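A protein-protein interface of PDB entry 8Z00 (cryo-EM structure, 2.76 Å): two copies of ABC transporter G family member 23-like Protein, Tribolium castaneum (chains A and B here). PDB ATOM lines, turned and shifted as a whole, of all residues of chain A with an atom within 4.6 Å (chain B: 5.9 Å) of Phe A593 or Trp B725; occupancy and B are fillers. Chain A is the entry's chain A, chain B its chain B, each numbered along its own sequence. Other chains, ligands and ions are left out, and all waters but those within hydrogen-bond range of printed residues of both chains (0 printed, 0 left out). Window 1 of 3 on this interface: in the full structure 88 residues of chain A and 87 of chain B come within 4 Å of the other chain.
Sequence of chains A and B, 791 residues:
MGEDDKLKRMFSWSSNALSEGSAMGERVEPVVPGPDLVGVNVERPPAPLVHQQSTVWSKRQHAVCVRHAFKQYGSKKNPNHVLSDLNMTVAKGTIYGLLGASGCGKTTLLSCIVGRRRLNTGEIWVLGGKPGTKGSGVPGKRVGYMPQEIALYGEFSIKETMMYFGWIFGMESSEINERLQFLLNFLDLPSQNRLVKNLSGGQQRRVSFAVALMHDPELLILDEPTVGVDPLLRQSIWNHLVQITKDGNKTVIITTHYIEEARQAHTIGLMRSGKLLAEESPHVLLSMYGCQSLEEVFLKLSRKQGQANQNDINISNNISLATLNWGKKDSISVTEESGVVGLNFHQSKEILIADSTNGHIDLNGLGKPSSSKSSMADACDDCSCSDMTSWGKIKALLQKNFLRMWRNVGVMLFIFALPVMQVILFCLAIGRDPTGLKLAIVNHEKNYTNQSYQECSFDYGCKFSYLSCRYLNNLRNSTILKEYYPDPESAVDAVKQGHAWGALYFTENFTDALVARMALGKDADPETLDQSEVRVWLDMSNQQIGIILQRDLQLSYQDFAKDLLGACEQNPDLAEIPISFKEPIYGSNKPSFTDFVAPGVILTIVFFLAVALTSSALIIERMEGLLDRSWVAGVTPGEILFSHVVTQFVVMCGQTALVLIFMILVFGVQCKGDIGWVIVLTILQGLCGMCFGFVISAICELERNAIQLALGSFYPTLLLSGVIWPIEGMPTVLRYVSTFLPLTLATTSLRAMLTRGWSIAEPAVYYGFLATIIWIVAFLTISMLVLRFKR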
ATOM      1  N   ALA A 429      32.365   7.080   4.368  1.00  0.00           N
ATOM      2  CA  ALA A 429      32.280   7.119   2.916  1.00  0.00           C
ATOM      3  C   ALA A 429      30.996   7.727   2.374  1.00  0.00           C
ATOM      4  O   ALA A 429      31.020   8.295   1.281  1.00  0.00           O
ATOM      5  CB  ALA A 429      32.431   5.705   2.337  1.00  0.00           C
ATOM      6  N   ILE A 430      29.883   7.631   3.097  1.00  0.00           N
ATOM      7  CA  ILE A 430      28.572   8.018   2.587  1.00  0.00           C
ATOM      8  C   ILE A 430      28.139   9.313   3.258  1.00  0.00           C
ATOM      9  O   ILE A 430      28.176   9.426   4.488  1.00  0.00           O
ATOM     10  CB  ILE A 430      27.531   6.909   2.818  1.00  0.00           C
ATOM     11  CG1 ILE A 430      28.115   5.543   2.453  1.00  0.00           C
ATOM     12  CG2 ILE A 430      26.269   7.187   2.018  1.00  0.00           C
ATOM     13  CD1 ILE A 430      28.385   5.364   0.980  1.00  0.00           C
ATOM     14  N   GLY A 431      27.730  10.289   2.445  1.00  0.00           N
ATOM     15  CA  GLY A 431      27.135  11.516   2.921  1.00  0.00           C
ATOM     16  C   GLY A 431      28.051  12.722   2.924  1.00  0.00           C
ATOM     17  O   GLY A 431      27.557  13.851   3.009  1.00  0.00           O
ATOM     18  N   ARG A 432      29.361  12.521   2.833  1.00  0.00           N
ATOM     19  CA  ARG A 432      30.290  13.637   2.891  1.00  0.00           C
ATOM     20  C   ARG A 432      30.353  14.363   1.549  1.00  0.00           C
ATOM     21  O   ARG A 432      29.935  13.847   0.510  1.00  0.00           O
ATOM     22  CB  ARG A 432      31.683  13.157   3.297  1.00  0.00           C
ATOM     23  CG  ARG A 432      31.775  12.695   4.739  1.00  0.00           C
ATOM     24  CD  ARG A 432      32.576  11.412   4.855  1.00  0.00           C
ATOM     25  NE  ARG A 432      33.943  11.658   5.297  1.00  0.00           N
ATOM     26  CZ  ARG A 432      34.300  11.850   6.560  1.00  0.00           C
ATOM     27  NH1 ARG A 432      33.412  11.831   7.539  1.00  0.00           N
ATOM     28  NH2 ARG A 432      35.581  12.065   6.846  1.00  0.00           N
ATOM     29  N   GLN A 544      25.491  15.434  -7.754  1.00  0.00           N
ATOM     30  CA  GLN A 544      25.952  15.980  -6.483  1.00  0.00           C
ATOM     31  C   GLN A 544      27.174  16.872  -6.648  1.00  0.00           C
ATOM     32  O   GLN A 544      27.358  17.813  -5.869  1.00  0.00           O
ATOM     33  CB  GLN A 544      26.252  14.849  -5.499  1.00  0.00           C
ATOM     34  CG  GLN A 544      25.048  13.986  -5.169  1.00  0.00           C
ATOM     35  CD  GLN A 544      23.972  14.743  -4.417  1.00  0.00           C
ATOM     36  OE1 GLN A 544      22.780  14.514  -4.617  1.00  0.00           O
ATOM     37  NE2 GLN A 544      24.388  15.651  -3.543  1.00  0.00           N
ATOM     38  N   PRO A 591      23.147  21.393   5.682  1.00  0.00           N
ATOM     39  CA  PRO A 591      22.662  20.050   6.015  1.00  0.00           C
ATOM     40  C   PRO A 591      23.588  18.973   5.469  1.00  0.00           C
ATOM     41  O   PRO A 591      24.345  19.181   4.519  1.00  0.00           O
ATOM     42  CB  PRO A 591      21.281  19.984   5.349  1.00  0.00           C
ATOM     43  CG  PRO A 591      20.991  21.370   4.846  1.00  0.00           C
ATOM     44  CD  PRO A 591      22.304  22.052   4.674  1.00  0.00           C
ATOM     45  N   SER A 592      23.517  17.802   6.095  1.00  0.00           N
ATOM     46  CA  SER A 592      24.345  16.663   5.731  1.00  0.00           C
ATOM     47  C   SER A 592      23.471  15.504   5.277  1.00  0.00           C
ATOM     48  O   SER A 592      22.411  15.248   5.857  1.00  0.00           O
ATOM     49  CB  SER A 592      25.225  16.221   6.902  1.00  0.00           C
ATOM     50  OG  SER A 592      26.402  15.586   6.437  1.00  0.00           O
ATOM     51  N   PHE A 593      23.916  14.812   4.229  1.00  0.00           N
ATOM     52  CA  PHE A 593      23.207  13.631   3.755  1.00  0.00           C
ATOM     53  C   PHE A 593      23.431  12.431   4.665  1.00  0.00           C
ATOM     54  O   PHE A 593      22.552  11.570   4.774  1.00  0.00           O
ATOM     55  CB  PHE A 593      23.635  13.293   2.328  1.00  0.00           C
ATOM     56  CG  PHE A 593      22.749  12.289   1.650  1.00  0.00           C
ATOM     57  CD1 PHE A 593      21.432  12.596   1.356  1.00  0.00           C
ATOM     58  CD2 PHE A 593      23.233  11.040   1.302  1.00  0.00           C
ATOM     59  CE1 PHE A 593      20.615  11.676   0.731  1.00  0.00           C
ATOM     60  CE2 PHE A 593      22.418  10.117   0.677  1.00  0.00           C
ATOM     61  CZ  PHE A 593      21.108  10.436   0.391  1.00  0.00           C
ATOM     62  N   THR A 594      24.592  12.351   5.318  1.00  0.00           N
ATOM     63  CA  THR A 594      24.852  11.257   6.244  1.00  0.00           C
ATOM     64  C   THR A 594      23.957  11.319   7.474  1.00  0.00           C
ATOM     65  O   THR A 594      23.774  10.298   8.143  1.00  0.00           O
ATOM     66  CB  THR A 594      26.326  11.255   6.660  1.00  0.00           C
ATOM     67  OG1 THR A 594      26.594  10.112   7.481  1.00  0.00           O
ATOM     68  CG2 THR A 594      26.667  12.516   7.429  1.00  0.00           C
ATOM     69  N   ASP A 595      23.397  12.489   7.785  1.00  0.00           N
ATOM     70  CA  ASP A 595      22.441  12.608   8.876  1.00  0.00           C
ATOM     71  C   ASP A 595      21.038  12.182   8.468  1.00  0.00           C
ATOM     72  O   ASP A 595      20.180  12.002   9.337  1.00  0.00           O
ATOM     73  CB  ASP A 595      22.412  14.045   9.395  1.00  0.00           C
ATOM     74  CG  ASP A 595      23.588  14.363  10.291  1.00  0.00           C
ATOM     75  OD1 ASP A 595      24.424  13.464  10.516  1.00  0.00           O
ATOM     76  OD2 ASP A 595      23.680  15.512  10.771  1.00  0.00           O
ATOM     77  N   PHE A 596      20.786  12.029   7.170  1.00  0.00           N
ATOM     78  CA  PHE A 596      19.497  11.564   6.675  1.00  0.00           C
ATOM     79  C   PHE A 596      19.428  10.045   6.610  1.00  0.00           C
ATOM     80  O   PHE A 596      18.386   9.458   6.918  1.00  0.00           O
ATOM     81  CB  PHE A 596      19.221  12.166   5.293  1.00  0.00           C
ATOM     82  CG  PHE A 596      18.008  11.598   4.611  1.00  0.00           C
ATOM     83  CD1 PHE A 596      16.746  12.090   4.891  1.00  0.00           C
ATOM     84  CD2 PHE A 596      18.131  10.580   3.681  1.00  0.00           C
ATOM     85  CE1 PHE A 596      15.632  11.571   4.264  1.00  0.00           C
ATOM     86  CE2 PHE A 596      17.023  10.058   3.054  1.00  0.00           C
ATOM     87  CZ  PHE A 596      15.772  10.554   3.345  1.00  0.00           C
ATOM     88  N   VAL A 597      20.524   9.396   6.217  1.00  0.00           N
ATOM     89  CA  VAL A 597      20.537   7.945   6.072  1.00  0.00           C
ATOM     90  C   VAL A 597      20.866   7.223   7.374  1.00  0.00           C
ATOM     91  O   VAL A 597      20.535   6.037   7.512  1.00  0.00           O
ATOM     92  CB  VAL A 597      21.531   7.528   4.971  1.00  0.00           C
ATOM     93  CG1 VAL A 597      21.208   6.137   4.451  1.00  0.00           C
ATOM     94  CG2 VAL A 597      21.509   8.533   3.835  1.00  0.00           C
ATOM     95  N   ILE A 724      17.453   5.461   1.846  1.00  0.00           N
ATOM     96  CA  ILE A 724      18.497   6.140   1.085  1.00  0.00           C
ATOM     97  C   ILE A 724      17.977   7.325   0.284  1.00  0.00           C
ATOM     98  O   ILE A 724      18.788   8.128  -0.205  1.00  0.00           O
ATOM     99  CB  ILE A 724      19.231   5.162   0.141  1.00  0.00           C
ATOM    100  CG1 ILE A 724      18.235   4.452  -0.775  1.00  0.00           C
ATOM    101  CG2 ILE A 724      20.037   4.151   0.940  1.00  0.00           C
ATOM    102  CD1 ILE A 724      18.876   3.457  -1.714  1.00  0.00           C
ATOM    103  N   GLN B 543      18.257  17.266   3.701  1.00  0.00           N
ATOM    104  CA  GLN B 543      19.225  17.880   2.797  1.00  0.00           C
ATOM    105  C   GLN B 543      18.661  18.034   1.389  1.00  0.00           C
ATOM    106  O   GLN B 543      18.793  19.096   0.771  1.00  0.00           O
ATOM    107  CB  GLN B 543      20.513  17.057   2.774  1.00  0.00           C
ATOM    108  CG  GLN B 543      21.746  17.852   2.377  1.00  0.00           C
ATOM    109  CD  GLN B 543      22.516  17.211   1.242  1.00  0.00           C
ATOM    110  OE1 GLN B 543      21.959  16.454   0.447  1.00  0.00           O
ATOM    111  NE2 GLN B 543      23.805  17.508   1.162  1.00  0.00           N
ATOM    112  N   GLN B 544      18.034  16.982   0.860  1.00  0.00           N
ATOM    113  CA  GLN B 544      17.566  17.026  -0.522  1.00  0.00           C
ATOM    114  C   GLN B 544      16.356  17.939  -0.674  1.00  0.00           C
ATOM    115  O   GLN B 544      16.222  18.635  -1.687  1.00  0.00           O
ATOM    116  CB  GLN B 544      17.241  15.617  -1.014  1.00  0.00           C
ATOM    117  CG  GLN B 544      18.454  14.714  -1.164  1.00  0.00           C
ATOM    118  CD  GLN B 544      19.560  15.345  -1.984  1.00  0.00           C
ATOM    119  OE1 GLN B 544      19.323  15.858  -3.077  1.00  0.00           O
ATOM    120  NE2 GLN B 544      20.779  15.311  -1.459  1.00  0.00           N
ATOM    121  N   PHE B 593      19.658  11.950  -9.918  1.00  0.00           N
ATOM    122  CA  PHE B 593      20.386  11.026  -9.057  1.00  0.00           C
ATOM    123  C   PHE B 593      20.159   9.574  -9.450  1.00  0.00           C
ATOM    124  O   PHE B 593      20.996   8.722  -9.130  1.00  0.00           O
ATOM    125  CB  PHE B 593      19.990  11.241  -7.596  1.00  0.00           C
ATOM    126  CG  PHE B 593      20.971  10.669  -6.614  1.00  0.00           C
ATOM    127  CD1 PHE B 593      22.279  11.121  -6.581  1.00  0.00           C
ATOM    128  CD2 PHE B 593      20.586   9.682  -5.725  1.00  0.00           C
ATOM    129  CE1 PHE B 593      23.183  10.597  -5.680  1.00  0.00           C
ATOM    130  CE2 PHE B 593      21.487   9.155  -4.823  1.00  0.00           C
ATOM    131  CZ  PHE B 593      22.787   9.614  -4.801  1.00  0.00           C
ATOM    132  N   PHE B 596      23.002   8.469 -11.693  1.00  0.00           N
ATOM    133  CA  PHE B 596      24.281   8.213 -11.040  1.00  0.00           C
ATOM    134  C   PHE B 596      24.321   6.829 -10.404  1.00  0.00           C
ATOM    135  O   PHE B 596      25.335   6.129 -10.494  1.00  0.00           O
ATOM    136  CB  PHE B 596      24.558   9.294  -9.993  1.00  0.00           C
ATOM    137  CG  PHE B 596      25.745   9.006  -9.118  1.00  0.00           C
ATOM    138  CD1 PHE B 596      27.029   9.272  -9.560  1.00  0.00           C
ATOM    139  CD2 PHE B 596      25.577   8.474  -7.852  1.00  0.00           C
ATOM    140  CE1 PHE B 596      28.119   9.006  -8.759  1.00  0.00           C
ATOM    141  CE2 PHE B 596      26.661   8.206  -7.050  1.00  0.00           C
ATOM    142  CZ  PHE B 596      27.934   8.473  -7.503  1.00  0.00           C
ATOM    143  N   SER B 721      32.617   1.137  -3.021  1.00  0.00           N
ATOM    144  CA  SER B 721      32.762   1.090  -4.470  1.00  0.00           C
ATOM    145  C   SER B 721      32.133   2.287  -5.170  1.00  0.00           C
ATOM    146  O   SER B 721      32.107   2.324  -6.404  1.00  0.00           O
ATOM    147  CB  SER B 721      32.167  -0.208  -5.017  1.00  0.00           C
ATOM    148  OG  SER B 721      30.759  -0.125  -5.109  1.00  0.00           O
ATOM    149  N   GLY B 722      31.635   3.263  -4.419  1.00  0.00           N
ATOM    150  CA  GLY B 722      31.050   4.451  -5.017  1.00  0.00           C
ATOM    151  C   GLY B 722      29.787   4.207  -5.816  1.00  0.00           C
ATOM    152  O   GLY B 722      29.627   4.777  -6.902  1.00  0.00           O
ATOM    153  N   VAL B 723      28.881   3.380  -5.303  1.00  0.00           N
ATOM    154  CA  VAL B 723      27.633   3.084  -5.998  1.00  0.00           C
ATOM    155  C   VAL B 723      26.535   4.067  -5.613  1.00  0.00           C
ATOM    156  O   VAL B 723      25.837   4.605  -6.477  1.00  0.00           O
ATOM    157  CB  VAL B 723      27.208   1.626  -5.721  1.00  0.00           C
ATOM    158  CG1 VAL B 723      25.720   1.442  -5.971  1.00  0.00           C
ATOM    159  CG2 VAL B 723      28.015   0.669  -6.576  1.00  0.00           C
ATOM    160  N   ILE B 724      26.367   4.325  -4.314  1.00  0.00           N
ATOM    161  CA  ILE B 724      25.290   5.189  -3.838  1.00  0.00           C
ATOM    162  C   ILE B 724      25.752   6.609  -3.539  1.00  0.00           C
ATOM    163  O   ILE B 724      24.903   7.503  -3.389  1.00  0.00           O
ATOM    164  CB  ILE B 724      24.606   4.594  -2.589  1.00  0.00           C
ATOM    165  CG1 ILE B 724      25.648   4.048  -1.613  1.00  0.00           C
ATOM    166  CG2 ILE B 724      23.629   3.503  -2.987  1.00  0.00           C
ATOM    167  CD1 ILE B 724      25.137   3.903  -0.199  1.00  0.00           C
ATOM    168  N   TRP B 725      27.054   6.848  -3.439  1.00  0.00           N
ATOM    169  CA  TRP B 725      27.588   8.180  -3.207  1.00  0.00           C
ATOM    170  C   TRP B 725      28.845   8.362  -4.042  1.00  0.00           C
ATOM    171  O   TRP B 725      29.559   7.388  -4.310  1.00  0.00           O
ATOM    172  CB  TRP B 725      27.903   8.410  -1.719  1.00  0.00           C
ATOM    173  CG  TRP B 725      28.097   9.853  -1.356  1.00  0.00           C
ATOM    174  CD1 TRP B 725      29.256  10.447  -0.957  1.00  0.00           C
ATOM    175  CD2 TRP B 725      27.103  10.884  -1.373  1.00  0.00           C
ATOM    176  NE1 TRP B 725      29.047  11.783  -0.721  1.00  0.00           N
ATOM    177  CE2 TRP B 725      27.732  12.076  -0.970  1.00  0.00           C
ATOM    178  CE3 TRP B 725      25.742  10.915  -1.690  1.00  0.00           C
ATOM    179  CZ2 TRP B 725      27.049  13.283  -0.873  1.00  0.00           C
ATOM    180  CZ3 TRP B 725      25.066  12.114  -1.594  1.00  0.00           C
ATOM    181  CH2 TRP B 725      25.719  13.282  -1.189  1.00  0.00           C
ATOM    182  N   PRO B 726      29.132   9.589  -4.482  1.00  0.00           N
ATOM    183  CA  PRO B 726      30.371   9.829  -5.231  1.00  0.00           C
ATOM    184  C   PRO B 726      31.605   9.429  -4.435  1.00  0.00           C
ATOM    185  O   PRO B 726      31.674   9.613  -3.220  1.00  0.00           O
ATOM    186  CB  PRO B 726      30.338  11.339  -5.487  1.00  0.00           C
ATOM    187  CG  PRO B 726      28.899  11.676  -5.516  1.00  0.00           C
ATOM    188  CD  PRO B 726      28.204  10.729  -4.575  1.00  0.00           C
ATOM    189  N   ILE B 727      32.589   8.871  -5.145  1.00  0.00           N
ATOM    190  CA  ILE B 727      33.831   8.431  -4.520  1.00  0.00           C
ATOM    191  C   ILE B 727      34.682   9.592  -4.033  1.00  0.00           C
ATOM    192  O   ILE B 727      35.603   9.384  -3.236  1.00  0.00           O
ATOM    193  CB  ILE B 727      34.633   7.555  -5.507  1.00  0.00           C
ATOM    194  CG1 ILE B 727      35.589   6.626  -4.761  1.00  0.00           C
ATOM    195  CG2 ILE B 727      35.401   8.416  -6.497  1.00  0.00           C
ATOM    196  CD1 ILE B 727      34.994   5.276  -4.444  1.00  0.00           C
ATOM    197  N   GLY B 729      33.875  11.962  -2.033  1.00  0.00           N
ATOM    198  CA  GLY B 729      33.614  12.334  -0.656  1.00  0.00           C
ATOM    199  C   GLY B 729      34.386  11.551   0.381  1.00  0.00           C
ATOM    200  O   GLY B 729      34.319  11.888   1.566  1.00  0.00           O
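Among the printed residues, merely in contact across the chains: Ala A429 with Trp B725 (3.6 Å), Ile A430 with Ile B724 (3.8 Å), Gly A431 with Trp B725 (3.7 Å), Arg A432 with Gly B729 (3.4 Å), Gln A544 with Gln B544 (3.8 Å), Gln A544 with Phe B593 (3.9 Å), Gln A544 with Trp B725 (3.6 Å), Pro A591 with Gln B543 (3.6 Å), Phe A593 with Gln B543 (3.999 Å), Phe A593 with Gln B544 (3.97 Å) and Phe A593 with Trp B725 (3.6 Å).
The indole nitrogen (NE1) of Trp B725 is in hydrogen-bond range of the backbone carbonyl oxygen (O) of Arg A432, 2.6 Å away.
O of Ile A430 lies close to OG1 of Thr A594, 3.5 Å away.
The side-chain amide oxygen (OE1) of Gln B543 is in hydrogen-bond range of the side-chain amide nitrogen (NE2) of Gln B544 (2.5 Å).
Printed residues of chain B within 4 Å of Gln A544: Gln B544, Phe B593 and Trp B725.
Printed residues of chain B within 4 Å of Pro A591: Gln B543.
Printed residues of chain B within 4 Å of Phe A593: Gln B543, Gln B544 and Trp B725.
Phe A596 touches none of the printed residues of chain B.
Of the printed residues of chain A, Gln B543 touches Pro A591 (3.6 Å) and Phe A593 (3.999 Å).
Printed residues of chain A within 4 Å of Gln B544: Gln A544 (3.8 Å) and Phe A593 (3.97 Å).
Gly B722 touches none of the printed residues of chain A.
Trp B725 touches five residues of chain A.
The nearest printed residue of chain B that does not touch Phe A593 is Phe B593 (5.4 Å).
The nearest residue of chain A that does not touch Trp B725 is Ile A430 (4.1 Å).
Gln B544 touches its own counterpart, Gln A544.
Gln A544 touches Phe B593, and with the chains exchanged Phe A593 touches Gln B544.
Positions printed for both chains: 544, 593, 596 and 724.
Printed residues of chain A that touch a printed residue of chain B: Ala A429, Ile A430, Gly A431, Arg A432, Gln A544, Pro A591 and Phe A593.
Hydrophobic or aromatic side chains of chain A that line the printed part of chain B: Ile A430, Pro A591 and Phe A593.
Hydrophobic or aromatic side chains of chain B within 4 Å of the printed part of chain A: Phe B593, Ile B724 and Trp B725.
Among the printed residues, no Asp or Glu carboxylate lies within 4 Å of a Lys or Arg side-chain nitrogen of the other chain.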
